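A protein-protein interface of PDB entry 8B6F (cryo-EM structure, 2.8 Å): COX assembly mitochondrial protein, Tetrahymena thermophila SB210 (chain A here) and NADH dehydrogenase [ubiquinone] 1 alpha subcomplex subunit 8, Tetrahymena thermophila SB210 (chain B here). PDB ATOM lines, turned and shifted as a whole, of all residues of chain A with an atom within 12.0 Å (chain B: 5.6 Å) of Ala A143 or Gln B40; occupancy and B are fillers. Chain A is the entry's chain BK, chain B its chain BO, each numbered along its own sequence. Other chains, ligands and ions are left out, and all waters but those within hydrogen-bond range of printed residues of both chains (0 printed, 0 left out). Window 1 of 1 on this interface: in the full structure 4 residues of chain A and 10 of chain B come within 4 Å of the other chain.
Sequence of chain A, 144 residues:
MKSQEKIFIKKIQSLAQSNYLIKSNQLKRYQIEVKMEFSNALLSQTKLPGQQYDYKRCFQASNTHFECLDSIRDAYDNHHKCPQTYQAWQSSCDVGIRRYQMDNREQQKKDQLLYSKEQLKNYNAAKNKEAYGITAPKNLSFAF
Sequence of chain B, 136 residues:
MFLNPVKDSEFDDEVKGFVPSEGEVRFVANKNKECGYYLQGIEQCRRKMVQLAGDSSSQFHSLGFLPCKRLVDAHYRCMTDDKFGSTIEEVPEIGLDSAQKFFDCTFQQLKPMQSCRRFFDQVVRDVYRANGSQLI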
ATOM      1  N   ALA A 136     -23.690 -26.661   2.559  1.00  0.00           N
ATOM      2  CA  ALA A 136     -24.828 -26.512   1.674  1.00  0.00           C
ATOM      3  C   ALA A 136     -25.401 -25.102   1.790  1.00  0.00           C
ATOM      4  O   ALA A 136     -25.307 -24.473   2.846  1.00  0.00           O
ATOM      5  CB  ALA A 136     -25.906 -27.536   2.010  1.00  0.00           C
ATOM      6  N   PRO A 137     -25.995 -24.581   0.721  1.00  0.00           N
ATOM      7  CA  PRO A 137     -26.593 -23.246   0.803  1.00  0.00           C
ATOM      8  C   PRO A 137     -27.792 -23.231   1.736  1.00  0.00           C
ATOM      9  O   PRO A 137     -28.505 -24.224   1.889  1.00  0.00           O
ATOM     10  CB  PRO A 137     -27.007 -22.952  -0.644  1.00  0.00           C
ATOM     11  CG  PRO A 137     -27.203 -24.290  -1.254  1.00  0.00           C
ATOM     12  CD  PRO A 137     -26.202 -25.197  -0.601  1.00  0.00           C
ATOM     13  N   LYS A 138     -28.003 -22.080   2.368  1.00  0.00           N
ATOM     14  CA  LYS A 138     -29.165 -21.854   3.225  1.00  0.00           C
ATOM     15  C   LYS A 138     -30.212 -21.128   2.390  1.00  0.00           C
ATOM     16  O   LYS A 138     -30.105 -19.925   2.145  1.00  0.00           O
ATOM     17  CB  LYS A 138     -28.789 -21.058   4.469  1.00  0.00           C
ATOM     18  CG  LYS A 138     -27.946 -21.834   5.466  1.00  0.00           C
ATOM     19  CD  LYS A 138     -27.803 -21.064   6.766  1.00  0.00           C
ATOM     20  CE  LYS A 138     -26.876 -21.772   7.738  1.00  0.00           C
ATOM     21  NZ  LYS A 138     -27.411 -23.097   8.153  1.00  0.00           N
ATOM     22  N   ASN A 139     -31.226 -21.865   1.952  1.00  0.00           N
ATOM     23  CA  ASN A 139     -32.270 -21.305   1.112  1.00  0.00           C
ATOM     24  C   ASN A 139     -33.362 -20.684   1.972  1.00  0.00           C
ATOM     25  O   ASN A 139     -33.622 -21.125   3.094  1.00  0.00           O
ATOM     26  CB  ASN A 139     -32.868 -22.382   0.207  1.00  0.00           C
ATOM     27  CG  ASN A 139     -31.816 -23.119  -0.594  1.00  0.00           C
ATOM     28  OD1 ASN A 139     -31.298 -22.604  -1.584  1.00  0.00           O
ATOM     29  ND2 ASN A 139     -31.498 -24.336  -0.174  1.00  0.00           N
ATOM     30  N   LEU A 140     -33.999 -19.647   1.432  1.00  0.00           N
ATOM     31  CA  LEU A 140     -35.084 -18.950   2.117  1.00  0.00           C
ATOM     32  C   LEU A 140     -34.612 -18.428   3.476  1.00  0.00           C
ATOM     33  O   LEU A 140     -35.099 -18.825   4.535  1.00  0.00           O
ATOM     34  CB  LEU A 140     -36.311 -19.858   2.261  1.00  0.00           C
ATOM     35  CG  LEU A 140     -37.157 -20.074   0.999  1.00  0.00           C
ATOM     36  CD1 LEU A 140     -36.335 -20.627  -0.150  1.00  0.00           C
ATOM     37  CD2 LEU A 140     -38.326 -20.995   1.292  1.00  0.00           C
ATOM     38  N   SER A 141     -33.637 -17.528   3.419  1.00  0.00           N
ATOM     39  CA  SER A 141     -33.084 -16.933   4.623  1.00  0.00           C
ATOM     40  C   SER A 141     -34.063 -15.914   5.202  1.00  0.00           C
ATOM     41  O   SER A 141     -35.134 -15.652   4.650  1.00  0.00           O
ATOM     42  CB  SER A 141     -31.739 -16.279   4.317  1.00  0.00           C
ATOM     43  OG  SER A 141     -31.207 -15.638   5.464  1.00  0.00           O
ATOM     44  N   PHE A 142     -33.685 -15.336   6.342  1.00  0.00           N
ATOM     45  CA  PHE A 142     -34.498 -14.338   7.016  1.00  0.00           C
ATOM     46  C   PHE A 142     -33.837 -12.973   7.120  1.00  0.00           C
ATOM     47  O   PHE A 142     -34.552 -11.976   7.261  1.00  0.00           O
ATOM     48  CB  PHE A 142     -34.864 -14.810   8.432  1.00  0.00           C
ATOM     49  CG  PHE A 142     -33.674 -15.080   9.304  1.00  0.00           C
ATOM     50  CD1 PHE A 142     -33.096 -14.063  10.042  1.00  0.00           C
ATOM     51  CD2 PHE A 142     -33.136 -16.353   9.390  1.00  0.00           C
ATOM     52  CE1 PHE A 142     -32.003 -14.307  10.848  1.00  0.00           C
ATOM     53  CE2 PHE A 142     -32.042 -16.604  10.194  1.00  0.00           C
ATOM     54  CZ  PHE A 142     -31.476 -15.579  10.924  1.00  0.00           C
ATOM     55  N   ALA A 143     -32.514 -12.897   7.057  1.00  0.00           N
ATOM     56  CA  ALA A 143     -31.800 -11.641   7.213  1.00  0.00           C
ATOM     57  C   ALA A 143     -31.506 -11.010   5.857  1.00  0.00           C
ATOM     58  O   ALA A 143     -31.462 -11.683   4.825  1.00  0.00           O
ATOM     59  CB  ALA A 143     -30.497 -11.856   7.983  1.00  0.00           C
ATOM     60  N   PHE A 144     -31.309  -9.695   5.876  1.00  0.00           N
ATOM     61  CA  PHE A 144     -30.974  -8.938   4.676  1.00  0.00           C
ATOM     62  C   PHE A 144     -32.073  -9.031   3.622  1.00  0.00           C
ATOM     63  O   PHE A 144     -32.987  -9.852   3.714  1.00  0.00           O
ATOM     64  CB  PHE A 144     -29.647  -9.429   4.092  1.00  0.00           C
ATOM     65  CG  PHE A 144     -28.487  -9.298   5.034  1.00  0.00           C
ATOM     66  CD1 PHE A 144     -28.190 -10.309   5.932  1.00  0.00           C
ATOM     67  CD2 PHE A 144     -27.695  -8.162   5.021  1.00  0.00           C
ATOM     68  CE1 PHE A 144     -27.122 -10.191   6.801  1.00  0.00           C
ATOM     69  CE2 PHE A 144     -26.628  -8.036   5.888  1.00  0.00           C
ATOM     70  CZ  PHE A 144     -26.339  -9.053   6.778  1.00  0.00           C
ATOM     71  OXT PHE A 144     -32.074  -8.275   2.649  1.00  0.00           O
ATOM     72  N   GLY B  36     -29.114  -6.052   8.533  1.00  0.00           N
ATOM     73  CA  GLY B  36     -29.247  -7.498   8.538  1.00  0.00           C
ATOM     74  C   GLY B  36     -28.208  -8.207   9.379  1.00  0.00           C
ATOM     75  O   GLY B  36     -28.443  -9.337   9.817  1.00  0.00           O
ATOM     76  N   TYR B  37     -27.063  -7.568   9.615  1.00  0.00           N
ATOM     77  CA  TYR B  37     -26.040  -8.170  10.463  1.00  0.00           C
ATOM     78  C   TYR B  37     -26.564  -8.407  11.871  1.00  0.00           C
ATOM     79  O   TYR B  37     -26.281  -9.441  12.485  1.00  0.00           O
ATOM     80  CB  TYR B  37     -24.806  -7.269  10.487  1.00  0.00           C
ATOM     81  CG  TYR B  37     -23.706  -7.731  11.408  1.00  0.00           C
ATOM     82  CD1 TYR B  37     -22.802  -8.702  11.005  1.00  0.00           C
ATOM     83  CD2 TYR B  37     -23.555  -7.177  12.670  1.00  0.00           C
ATOM     84  CE1 TYR B  37     -21.788  -9.120  11.838  1.00  0.00           C
ATOM     85  CE2 TYR B  37     -22.543  -7.588  13.511  1.00  0.00           C
ATOM     86  CZ  TYR B  37     -21.662  -8.559  13.088  1.00  0.00           C
ATOM     87  OH  TYR B  37     -20.654  -8.973  13.919  1.00  0.00           O
ATOM     88  N   TYR B  38     -27.331  -7.454  12.402  1.00  0.00           N
ATOM     89  CA  TYR B  38     -27.827  -7.570  13.767  1.00  0.00           C
ATOM     90  C   TYR B  38     -28.796  -8.736  13.916  1.00  0.00           C
ATOM     91  O   TYR B  38     -28.805  -9.413  14.949  1.00  0.00           O
ATOM     92  CB  TYR B  38     -28.496  -6.264  14.186  1.00  0.00           C
ATOM     93  CG  TYR B  38     -27.545  -5.096  14.299  1.00  0.00           C
ATOM     94  CD1 TYR B  38     -26.310  -5.235  14.919  1.00  0.00           C
ATOM     95  CD2 TYR B  38     -27.880  -3.855  13.779  1.00  0.00           C
ATOM     96  CE1 TYR B  38     -25.439  -4.173  15.024  1.00  0.00           C
ATOM     97  CE2 TYR B  38     -27.015  -2.784  13.878  1.00  0.00           C
ATOM     98  CZ  TYR B  38     -25.796  -2.949  14.501  1.00  0.00           C
ATOM     99  OH  TYR B  38     -24.932  -1.885  14.602  1.00  0.00           O
ATOM    100  N   LEU B  39     -29.619  -8.989  12.897  1.00  0.00           N
ATOM    101  CA  LEU B  39     -30.586 -10.077  12.991  1.00  0.00           C
ATOM    102  C   LEU B  39     -29.888 -11.431  12.989  1.00  0.00           C
ATOM    103  O   LEU B  39     -30.228 -12.311  13.787  1.00  0.00           O
ATOM    104  CB  LEU B  39     -31.592  -9.985  11.844  1.00  0.00           C
ATOM    105  CG  LEU B  39     -32.854 -10.844  11.970  1.00  0.00           C
ATOM    106  CD1 LEU B  39     -33.688 -10.437  13.178  1.00  0.00           C
ATOM    107  CD2 LEU B  39     -33.677 -10.752  10.702  1.00  0.00           C
ATOM    108  N   GLN B  40     -28.913 -11.617  12.101  1.00  0.00           N
ATOM    109  CA  GLN B  40     -28.125 -12.844  12.124  1.00  0.00           C
ATOM    110  C   GLN B  40     -27.392 -12.983  13.449  1.00  0.00           C
ATOM    111  O   GLN B  40     -27.284 -14.084  13.998  1.00  0.00           O
ATOM    112  CB  GLN B  40     -27.138 -12.858  10.958  1.00  0.00           C
ATOM    113  CG  GLN B  40     -26.487 -14.212  10.721  1.00  0.00           C
ATOM    114  CD  GLN B  40     -27.450 -15.237  10.161  1.00  0.00           C
ATOM    115  OE1 GLN B  40     -27.582 -16.337  10.694  1.00  0.00           O
ATOM    116  NE2 GLN B  40     -28.126 -14.884   9.074  1.00  0.00           N
ATOM    117  N   GLY B  41     -26.886 -11.871  13.978  1.00  0.00           N
ATOM    118  CA  GLY B  41     -26.269 -11.901  15.292  1.00  0.00           C
ATOM    119  C   GLY B  41     -27.232 -12.331  16.379  1.00  0.00           C
ATOM    120  O   GLY B  41     -26.862 -13.070  17.294  1.00  0.00           O
ATOM    121  N   ILE B  42     -28.479 -11.867  16.303  1.00  0.00           N
ATOM    122  CA  ILE B  42     -29.474 -12.268  17.292  1.00  0.00           C
ATOM    123  C   ILE B  42     -29.701 -13.772  17.231  1.00  0.00           C
ATOM    124  O   ILE B  42     -29.768 -14.445  18.266  1.00  0.00           O
ATOM    125  CB  ILE B  42     -30.782 -11.483  17.075  1.00  0.00           C
ATOM    126  CG1 ILE B  42     -30.592 -10.021  17.484  1.00  0.00           C
ATOM    127  CG2 ILE B  42     -31.926 -12.101  17.872  1.00  0.00           C
ATOM    128  CD1 ILE B  42     -31.715  -9.109  17.041  1.00  0.00           C
ATOM    129  N   GLU B  43     -29.835 -14.324  16.024  1.00  0.00           N
ATOM    130  CA  GLU B  43     -30.026 -15.764  15.895  1.00  0.00           C
ATOM    131  C   GLU B  43     -28.842 -16.524  16.477  1.00  0.00           C
ATOM    132  O   GLU B  43     -29.013 -17.437  17.292  1.00  0.00           O
ATOM    133  CB  GLU B  43     -30.214 -16.139  14.426  1.00  0.00           C
ATOM    134  CG  GLU B  43     -30.671 -17.574  14.226  1.00  0.00           C
ATOM    135  CD  GLU B  43     -30.381 -18.099  12.834  1.00  0.00           C
ATOM    136  OE1 GLU B  43     -29.516 -17.522  12.144  1.00  0.00           O
ATOM    137  OE2 GLU B  43     -31.017 -19.094  12.427  1.00  0.00           O
ATOM    138  N   GLN B  44     -27.627 -16.164  16.057  1.00  0.00           N
ATOM    139  CA  GLN B  44     -26.446 -16.892  16.503  1.00  0.00           C
ATOM    140  C   GLN B  44     -26.270 -16.774  18.009  1.00  0.00           C
ATOM    141  O   GLN B  44     -25.932 -17.754  18.683  1.00  0.00           O
ATOM    142  CB  GLN B  44     -25.207 -16.372  15.776  1.00  0.00           C
ATOM    143  CG  GLN B  44     -25.263 -16.536  14.265  1.00  0.00           C
ATOM    144  CD  GLN B  44     -25.290 -17.984  13.829  1.00  0.00           C
ATOM    145  OE1 GLN B  44     -24.980 -18.885  14.605  1.00  0.00           O
ATOM    146  NE2 GLN B  44     -25.670 -18.216  12.579  1.00  0.00           N
ATOM    147  N   CYS B  45     -26.495 -15.579  18.556  1.00  0.00           N
ATOM    148  CA  CYS B  45     -26.349 -15.385  19.993  1.00  0.00           C
ATOM    149  C   CYS B  45     -27.442 -16.105  20.770  1.00  0.00           C
ATOM    150  O   CYS B  45     -27.185 -16.607  21.868  1.00  0.00           O
ATOM    151  CB  CYS B  45     -26.359 -13.894  20.328  1.00  0.00           C
ATOM    152  SG  CYS B  45     -26.028 -13.533  22.064  1.00  0.00           S
ATOM    153  N   ARG B 117     -38.798 -12.084  12.563  1.00  0.00           N
ATOM    154  CA  ARG B 117     -38.526 -10.884  11.779  1.00  0.00           C
ATOM    155  C   ARG B 117     -39.814 -10.219  11.323  1.00  0.00           C
ATOM    156  O   ARG B 117     -39.857  -8.995  11.156  1.00  0.00           O
ATOM    157  CB  ARG B 117     -37.657 -11.216  10.566  1.00  0.00           C
ATOM    158  CG  ARG B 117     -37.741 -10.161   9.467  1.00  0.00           C
ATOM    159  CD  ARG B 117     -36.645 -10.315   8.434  1.00  0.00           C
ATOM    160  NE  ARG B 117     -36.791  -9.344   7.354  1.00  0.00           N
ATOM    161  CZ  ARG B 117     -35.888  -9.130   6.407  1.00  0.00           C
ATOM    162  NH1 ARG B 117     -34.743  -9.791   6.381  1.00  0.00           N
ATOM    163  NH2 ARG B 117     -36.143  -8.232   5.459  1.00  0.00           N
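O of Phe A142 lies close to NE of Arg B117, 3.5 Å away.
O of Phe A144 lies within salt-bridge range of NH1 of Arg B117.
The backbone NH (N) of Ala A143 lies within hydrogen-bond range of the side-chain hydroxyl (OG) of Ser A141 (3.4 Å).
OE1 of Gln B40 sits close to OE1 of Glu B43 (2.7 Å).
NE2 of Gln B44 lies within hydrogen-bond range of OE1 of Gln B40 (3.3 Å).
Among the printed residues, merely in contact across the chains: Phe A142 with Glu B43 (3.0 Å), Phe A144 with Tyr B37 (3.3 Å), Phe A144 with Gly B36 (3.3 Å), Phe A142 with Leu B39 (3.4 Å), Ala A143 with Arg B117 (3.5 Å), Ala A143 with Gly B36 (3.7 Å), Phe A142 with Gln B40 (3.9 Å) and Ala A143 with Gln B40 (3.998 Å).
Printed residues of chain B within 4 Å of Ala A143: Gly B36 (3.7 Å), Gln B40 (3.998 Å) and Arg B117 (3.5 Å).
Of the printed residues of chain A, Gln B40 touches Phe A142 (3.9 Å) and Ala A143 (3.998 Å).
Of chain A, only Phe A144 (3.3 Å) comes within 4 Å of Tyr B37.
No residue of chain A comes within 4 Å of Gly B41.
No residue of chain A comes within 4 Å of Ile B42.
Glu B43 touches just one residue of chain A: Phe A142 (3.0 Å).
No residue of chain A comes within 4 Å of Gln B44.
Printed residues of chain A within 4 Å of Arg B117: Phe A142, Ala A143 and Phe A144.
Printed residues of chain B within 4 Å of Phe A142: Leu B39, Gln B40, Glu B43 and Arg B117.
Ser A141 touches none of the printed residues of chain B.
The nearest printed residue of chain B that does not touch Ala A143 is Leu B39 (4.1 Å).
The nearest printed residue of chain A that does not touch Gln B40 is Ser A141 (4.8 Å).
Printed residues of chain A that touch a printed residue of chain B: Phe A142, Ala A143 and Phe A144.
Hydrophobic or aromatic side chains of chain A that line the printed part of chain B: Phe A142, Ala A143 and Phe A144.
Along chain A the printed residues that touch a printed residue of chain B span positions 142 to 144.
Hydrophobic or aromatic side chains of chain B within 4 Å of the printed part of chain A: Leu B39.
Among the printed residues, 10 pairs touch across the chains.
Among the printed residues, no Asp or Glu carboxylate lies within 4 Å of a Lys or Arg side-chain nitrogen of the other chain.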
